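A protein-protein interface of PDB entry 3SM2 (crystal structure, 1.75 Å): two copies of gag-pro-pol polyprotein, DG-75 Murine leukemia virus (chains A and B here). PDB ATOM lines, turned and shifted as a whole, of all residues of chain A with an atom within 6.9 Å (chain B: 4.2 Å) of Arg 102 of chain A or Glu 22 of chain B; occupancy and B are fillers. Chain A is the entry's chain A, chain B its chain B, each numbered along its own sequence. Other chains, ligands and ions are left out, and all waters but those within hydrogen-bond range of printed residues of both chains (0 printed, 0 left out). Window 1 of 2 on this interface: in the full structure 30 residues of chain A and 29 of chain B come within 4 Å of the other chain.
CG of Pro 23 of chain B touches CB of Thr 40 of chain A (3.9 Å).
Gly 41 of chain A touches Leu 37 of chain B (CA to CD2, 3.8 Å).
Arg 102 of chain A touches Pro 21 of chain B.
O of Glu 22 of chain B touches CD of Arg 102 of chain A (3.3 Å).
No position is printed for both chains.
The backbone NH (N) of Ala 119 of chain B is in hydrogen-bond range of the side-chain carboxylate (OE2) of Glu 22 of chain B.
N of Arg 102 of chain A is in hydrogen-bond range of O of Ala 42 of chain A, 2.8 Å away.
The backbone carbonyl oxygen of Thr 40 of chain A is in hydrogen-bond range of the guanidinium group of Arg 102 of chain A.
The side-chain carboxylate (OD1) of Asp 39 of chain A lies within hydrogen-bond range of the backbone NH (N) of Gly 41 of chain A, 3.1 Å away.
The side-chain hydroxyl (OG1) of Thr 106 of chain A lies within hydrogen-bond range of the backbone carbonyl oxygen (O) of Arg 102 of chain A.
Of chain B, only Pro 21 (3.6 Å) and Glu 22 (3.3 Å) come within 4 Å of Arg 102 of chain A.
Of chain A, only Arg 102 comes within 4 Å of Glu 22 of chain B.
Printed residues of chain B within 4 Å of Thr 40 of chain A: Pro 23 (3.9 Å).
Of the printed residues of chain B, Gly 41 of chain A touches Leu 37 (3.8 Å).
The nearest residue of chain B that does not touch Arg 102 of chain A is Pro 23 of chain B (4.03 Å).
Of the 8 printed residues of chain B, 4 touch a printed residue of chain A.
Hydrophobic or aromatic side chains of chain B that line the printed part of chain A: Pro 21, Pro 23 and Leu 37.
Among the printed residues, 4 pairs touch across the chains.
Among the printed residues, no Asp or Glu carboxylate lies within 4 Å of a Lys or Arg side-chain nitrogen of the other chain.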
ATOM      1  N   ASP A  39      -7.088   1.635  -5.877  1.00  0.00           N
ATOM      2  CA  ASP A  39      -8.213   2.523  -6.224  1.00  0.00           C
ATOM      3  C   ASP A  39      -7.970   3.960  -5.776  1.00  0.00           C
ATOM      4  O   ASP A  39      -8.304   4.320  -4.647  1.00  0.00           O
ATOM      5  CB  ASP A  39      -9.521   2.011  -5.587  1.00  0.00           C
ATOM      6  CG  ASP A  39     -10.743   2.702  -6.140  1.00  0.00           C
ATOM      7  OD1 ASP A  39     -10.591   3.704  -6.898  1.00  0.00           O
ATOM      8  OD2 ASP A  39     -11.865   2.226  -5.838  1.00  0.00           O
ATOM      9  N   THR A  40      -7.390   4.776  -6.658  1.00  0.00           N
ATOM     10  CA  THR A  40      -7.049   6.169  -6.313  1.00  0.00           C
ATOM     11  C   THR A  40      -8.297   7.028  -6.112  1.00  0.00           C
ATOM     12  O   THR A  40      -8.213   8.101  -5.526  1.00  0.00           O
ATOM     13  CB  THR A  40      -6.122   6.823  -7.335  1.00  0.00           C
ATOM     14  OG1 THR A  40      -6.756   6.793  -8.635  1.00  0.00           O
ATOM     15  CG2 THR A  40      -4.770   6.074  -7.367  1.00  0.00           C
ATOM     16  N   GLY A  41      -9.446   6.546  -6.579  1.00  0.00           N
ATOM     17  CA  GLY A  41     -10.710   7.293  -6.403  1.00  0.00           C
ATOM     18  C   GLY A  41     -11.443   6.965  -5.123  1.00  0.00           C
ATOM     19  O   GLY A  41     -12.522   7.538  -4.868  1.00  0.00           O
ATOM     20  N   ALA A  42     -10.879   6.043  -4.332  1.00  0.00           N
ATOM     21  CA  ALA A  42     -11.483   5.624  -3.073  1.00  0.00           C
ATOM     22  C   ALA A  42     -10.785   6.324  -1.905  1.00  0.00           C
ATOM     23  O   ALA A  42      -9.569   6.199  -1.708  1.00  0.00           O
ATOM     24  CB  ALA A  42     -11.433   4.103  -2.922  1.00  0.00           C
ATOM     25  N   GLN A  43     -11.559   7.079  -1.145  1.00  0.00           N
ATOM     26  CA  GLN A  43     -10.995   7.789  -0.008  1.00  0.00           C
ATOM     27  C   GLN A  43     -10.541   6.797   1.072  1.00  0.00           C
ATOM     28  O   GLN A  43      -9.512   7.026   1.753  1.00  0.00           O
ATOM     29  CB  GLN A  43     -12.065   8.719   0.577  1.00  0.00           C
ATOM     30  CG  GLN A  43     -11.619   9.480   1.803  1.00  0.00           C
ATOM     31  CD  GLN A  43     -12.659  10.481   2.256  1.00  0.00           C
ATOM     32  OE1 GLN A  43     -13.691  10.676   1.606  1.00  0.00           O
ATOM     33  NE2 GLN A  43     -12.388  11.134   3.382  1.00  0.00           N
ATOM     34  N   HIS A  44     -11.329   5.742   1.289  1.00  0.00           N
ATOM     35  CA  HIS A  44     -10.949   4.743   2.307  1.00  0.00           C
ATOM     36  C   HIS A  44     -10.892   3.352   1.682  1.00  0.00           C
ATOM     37  O   HIS A  44     -11.529   3.082   0.667  1.00  0.00           O
ATOM     38  CB  HIS A  44     -11.863   4.643   3.535  1.00  0.00           C
ATOM     39  CG  HIS A  44     -11.109   4.297   4.790  1.00  0.00           C
ATOM     40  ND1 HIS A  44     -10.451   5.249   5.548  1.00  0.00           N
ATOM     41  CD2 HIS A  44     -10.821   3.101   5.360  1.00  0.00           C
ATOM     42  CE1 HIS A  44      -9.840   4.658   6.560  1.00  0.00           C
ATOM     43  NE2 HIS A  44     -10.046   3.356   6.467  1.00  0.00           N
ATOM     44  N   SER A  45     -10.155   2.468   2.328  1.00  0.00           N
ATOM     45  CA  SER A  45      -9.966   1.109   1.831  1.00  0.00           C
ATOM     46  C   SER A  45     -11.126   0.233   2.296  1.00  0.00           C
ATOM     47  O   SER A  45     -11.728   0.490   3.341  1.00  0.00           O
ATOM     48  CB  SER A  45      -8.639   0.560   2.332  1.00  0.00           C
ATOM     49  OG  SER A  45      -7.603   1.321   1.774  1.00  0.00           O
ATOM     50  N   LEU A 100      -8.018  -0.864  -2.364  1.00  0.00           N
ATOM     51  CA  LEU A 100      -6.917  -0.219  -1.666  1.00  0.00           C
ATOM     52  C   LEU A 100      -6.974   1.270  -2.028  1.00  0.00           C
ATOM     53  O   LEU A 100      -6.642   1.665  -3.141  1.00  0.00           O
ATOM     54  CB  LEU A 100      -5.560  -0.869  -2.024  1.00  0.00           C
ATOM     55  CG  LEU A 100      -4.416  -0.448  -1.082  1.00  0.00           C
ATOM     56  CD1 LEU A 100      -4.642  -1.055   0.267  1.00  0.00           C
ATOM     57  CD2 LEU A 100      -3.117  -0.949  -1.637  1.00  0.00           C
ATOM     58  N   GLY A 101      -7.456   2.083  -1.094  1.00  0.00           N
ATOM     59  CA  GLY A 101      -7.707   3.518  -1.384  1.00  0.00           C
ATOM     60  C   GLY A 101      -6.600   4.449  -0.935  1.00  0.00           C
ATOM     61  O   GLY A 101      -5.509   4.012  -0.582  1.00  0.00           O
ATOM     62  N   ARG A 102      -6.872   5.759  -0.969  1.00  0.00           N
ATOM     63  CA  ARG A 102      -5.843   6.754  -0.764  1.00  0.00           C
ATOM     64  C   ARG A 102      -5.322   6.723   0.664  1.00  0.00           C
ATOM     65  O   ARG A 102      -4.168   7.106   0.916  1.00  0.00           O
ATOM     66  CB  ARG A 102      -6.395   8.141  -1.097  1.00  0.00           C
ATOM     67  CG  ARG A 102      -6.811   8.273  -2.572  1.00  0.00           C
ATOM     68  CD  ARG A 102      -7.062   9.754  -2.936  1.00  0.00           C
ATOM     69  NE  ARG A 102      -8.167  10.351  -2.176  1.00  0.00           N
ATOM     70  CZ  ARG A 102      -9.445  10.331  -2.539  1.00  0.00           C
ATOM     71  NH1 ARG A 102      -9.837   9.739  -3.684  1.00  0.00           N
ATOM     72  NH2 ARG A 102     -10.347  10.902  -1.734  1.00  0.00           N
ATOM     73  N   ASP A 103      -6.177   6.300   1.599  1.00  0.00           N
ATOM     74  CA  ASP A 103      -5.741   6.203   3.001  1.00  0.00           C
ATOM     75  C   ASP A 103      -4.516   5.302   3.175  1.00  0.00           C
ATOM     76  O   ASP A 103      -3.646   5.608   3.986  1.00  0.00           O
ATOM     77  CB  ASP A 103      -6.892   5.761   3.895  1.00  0.00           C
ATOM     78  CG  ASP A 103      -7.505   4.418   3.471  1.00  0.00           C
ATOM     79  OD1 ASP A 103      -7.231   3.901   2.371  1.00  0.00           O
ATOM     80  OD2 ASP A 103      -8.327   3.886   4.242  1.00  0.00           O
ATOM     81  N   LEU A 104      -4.418   4.224   2.390  1.00  0.00           N
ATOM     82  CA  LEU A 104      -3.255   3.347   2.498  1.00  0.00           C
ATOM     83  C   LEU A 104      -2.216   3.618   1.428  1.00  0.00           C
ATOM     84  O   LEU A 104      -1.028   3.369   1.650  1.00  0.00           O
ATOM     85  CB  LEU A 104      -3.683   1.870   2.463  1.00  0.00           C
ATOM     86  CG  LEU A 104      -4.168   1.335   3.805  1.00  0.00           C
ATOM     87  CD1 LEU A 104      -4.887  -0.030   3.660  1.00  0.00           C
ATOM     88  CD2 LEU A 104      -3.022   1.271   4.831  1.00  0.00           C
ATOM     89  N   LEU A 105      -2.642   4.124   0.264  1.00  0.00           N
ATOM     90  CA  LEU A 105      -1.663   4.457  -0.782  1.00  0.00           C
ATOM     91  C   LEU A 105      -0.721   5.535  -0.283  1.00  0.00           C
ATOM     92  O   LEU A 105       0.452   5.543  -0.658  1.00  0.00           O
ATOM     93  CB  LEU A 105      -2.355   4.876  -2.118  1.00  0.00           C
ATOM     94  CG  LEU A 105      -3.123   3.756  -2.822  1.00  0.00           C
ATOM     95  CD1 LEU A 105      -4.015   4.264  -3.962  1.00  0.00           C
ATOM     96  CD2 LEU A 105      -2.170   2.712  -3.338  1.00  0.00           C
ATOM     97  N   THR A 106      -1.221   6.440   0.552  1.00  0.00           N
ATOM     98  CA  THR A 106      -0.387   7.512   1.065  1.00  0.00           C
ATOM     99  C   THR A 106       0.670   6.957   2.005  1.00  0.00           C
ATOM    100  O   THR A 106       1.780   7.485   2.056  1.00  0.00           O
ATOM    101  CB  THR A 106      -1.188   8.674   1.721  1.00  0.00           C
ATOM    102  OG1 THR A 106      -2.039   8.186   2.764  1.00  0.00           O
ATOM    103  CG2 THR A 106      -2.030   9.366   0.689  1.00  0.00           C
ATOM    104  N   LYS A 107       0.331   5.876   2.703  1.00  0.00           N
ATOM    105  CA  LYS A 107       1.270   5.248   3.642  1.00  0.00           C
ATOM    106  C   LYS A 107       2.287   4.445   2.871  1.00  0.00           C
ATOM    107  O   LYS A 107       3.477   4.490   3.178  1.00  0.00           O
ATOM    108  CB  LYS A 107       0.528   4.363   4.655  1.00  0.00           C
ATOM    109  CG  LYS A 107      -0.493   5.165   5.452  1.00  0.00           C
ATOM    110  CD  LYS A 107      -1.078   4.375   6.616  1.00  0.00           C
ATOM    111  CE  LYS A 107      -1.879   5.313   7.543  1.00  0.00           C
ATOM    112  NZ  LYS A 107      -3.045   4.614   8.156  1.00  0.00           N
ATOM    113  N   PRO B  20     -11.713  18.362  -7.242  1.00  0.00           N
ATOM    114  CA  PRO B  20     -11.606  17.010  -6.685  1.00  0.00           C
ATOM    115  C   PRO B  20     -10.338  16.840  -5.821  1.00  0.00           C
ATOM    116  O   PRO B  20      -9.384  17.615  -5.959  1.00  0.00           O
ATOM    117  CB  PRO B  20     -11.504  16.119  -7.933  1.00  0.00           C
ATOM    118  CG  PRO B  20     -11.799  16.981  -9.094  1.00  0.00           C
ATOM    119  CD  PRO B  20     -11.613  18.390  -8.714  1.00  0.00           C
ATOM    120  N   PRO B  21     -10.291  15.802  -4.969  1.00  0.00           N
ATOM    121  CA  PRO B  21      -9.062  15.542  -4.233  1.00  0.00           C
ATOM    122  C   PRO B  21      -7.938  15.133  -5.201  1.00  0.00           C
ATOM    123  O   PRO B  21      -8.215  14.772  -6.354  1.00  0.00           O
ATOM    124  CB  PRO B  21      -9.419  14.343  -3.329  1.00  0.00           C
ATOM    125  CG  PRO B  21     -10.783  13.923  -3.704  1.00  0.00           C
ATOM    126  CD  PRO B  21     -11.234  14.672  -4.898  1.00  0.00           C
ATOM    127  N   GLU B  22      -6.683  15.225  -4.754  1.00  0.00           N
ATOM    128  CA  GLU B  22      -5.581  14.637  -5.519  1.00  0.00           C
ATOM    129  C   GLU B  22      -5.673  13.108  -5.430  1.00  0.00           C
ATOM    130  O   GLU B  22      -6.152  12.569  -4.418  1.00  0.00           O
ATOM    131  CB  GLU B  22      -4.213  15.094  -4.972  1.00  0.00           C
ATOM    132  CG  GLU B  22      -4.002  16.588  -5.088  1.00  0.00           C
ATOM    133  CD  GLU B  22      -2.587  16.999  -4.694  1.00  0.00           C
ATOM    134  OE1 GLU B  22      -2.036  17.907  -5.359  1.00  0.00           O
ATOM    135  OE2 GLU B  22      -2.027  16.399  -3.750  1.00  0.00           O
ATOM    136  N   PRO B  23      -5.173  12.386  -6.436  1.00  0.00           N
ATOM    137  CA  PRO B  23      -4.537  12.850  -7.663  1.00  0.00           C
ATOM    138  C   PRO B  23      -5.572  13.415  -8.634  1.00  0.00           C
ATOM    139  O   PRO B  23      -6.634  12.816  -8.846  1.00  0.00           O
ATOM    140  CB  PRO B  23      -3.889  11.593  -8.225  1.00  0.00           C
ATOM    141  CG  PRO B  23      -4.703  10.432  -7.669  1.00  0.00           C
ATOM    142  CD  PRO B  23      -5.300  10.916  -6.372  1.00  0.00           C
ATOM    143  N   ARG B  24      -5.277  14.566  -9.222  1.00  0.00           N
ATOM    144  CA  ARG B  24      -6.222  15.153 -10.170  1.00  0.00           C
ATOM    145  C   ARG B  24      -5.506  15.725 -11.372  1.00  0.00           C
ATOM    146  O   ARG B  24      -4.310  16.026 -11.292  1.00  0.00           O
ATOM    147  CB  ARG B  24      -7.074  16.248  -9.497  1.00  0.00           C
ATOM    148  CG  ARG B  24      -6.273  17.365  -8.885  1.00  0.00           C
ATOM    149  CD  ARG B  24      -7.175  18.346  -8.148  1.00  0.00           C
ATOM    150  NE  ARG B  24      -6.355  19.385  -7.555  1.00  0.00           N
ATOM    151  CZ  ARG B  24      -6.232  19.603  -6.258  1.00  0.00           C
ATOM    152  NH1 ARG B  24      -6.930  18.896  -5.387  1.00  0.00           N
ATOM    153  NH2 ARG B  24      -5.435  20.574  -5.839  1.00  0.00           N
ATOM    154  N   LEU B  37     -10.904  13.849 -11.009  1.00  0.00           N
ATOM    155  CA  LEU B  37     -10.227  12.955 -10.079  1.00  0.00           C
ATOM    156  C   LEU B  37      -9.626  11.802 -10.870  1.00  0.00           C
ATOM    157  O   LEU B  37     -10.332  11.127 -11.643  1.00  0.00           O
ATOM    158  CB  LEU B  37     -11.229  12.425  -9.045  1.00  0.00           C
ATOM    159  CG  LEU B  37     -10.718  11.309  -8.123  1.00  0.00           C
ATOM    160  CD1 LEU B  37      -9.586  11.819  -7.285  1.00  0.00           C
ATOM    161  CD2 LEU B  37     -11.846  10.847  -7.244  1.00  0.00           C
ATOM    162  N   GLY B 118       1.020  14.749  -1.121  1.00  0.00           N
ATOM    163  CA  GLY B 118      -0.214  14.604  -1.875  1.00  0.00           C
ATOM    164  C   GLY B 118      -0.083  13.501  -2.914  1.00  0.00           C
ATOM    165  O   GLY B 118       0.566  12.477  -2.684  1.00  0.00           O
ATOM    166  N   ALA B 119      -0.710  13.699  -4.062  1.00  0.00           N
ATOM    167  CA  ALA B 119      -0.585  12.730  -5.129  1.00  0.00           C
ATOM    168  C   ALA B 119      -0.478  13.496  -6.431  1.00  0.00           C
ATOM    169  O   ALA B 119      -1.201  14.469  -6.622  1.00  0.00           O
ATOM    170  CB  ALA B 119      -1.783  11.778  -5.138  1.00  0.00           C
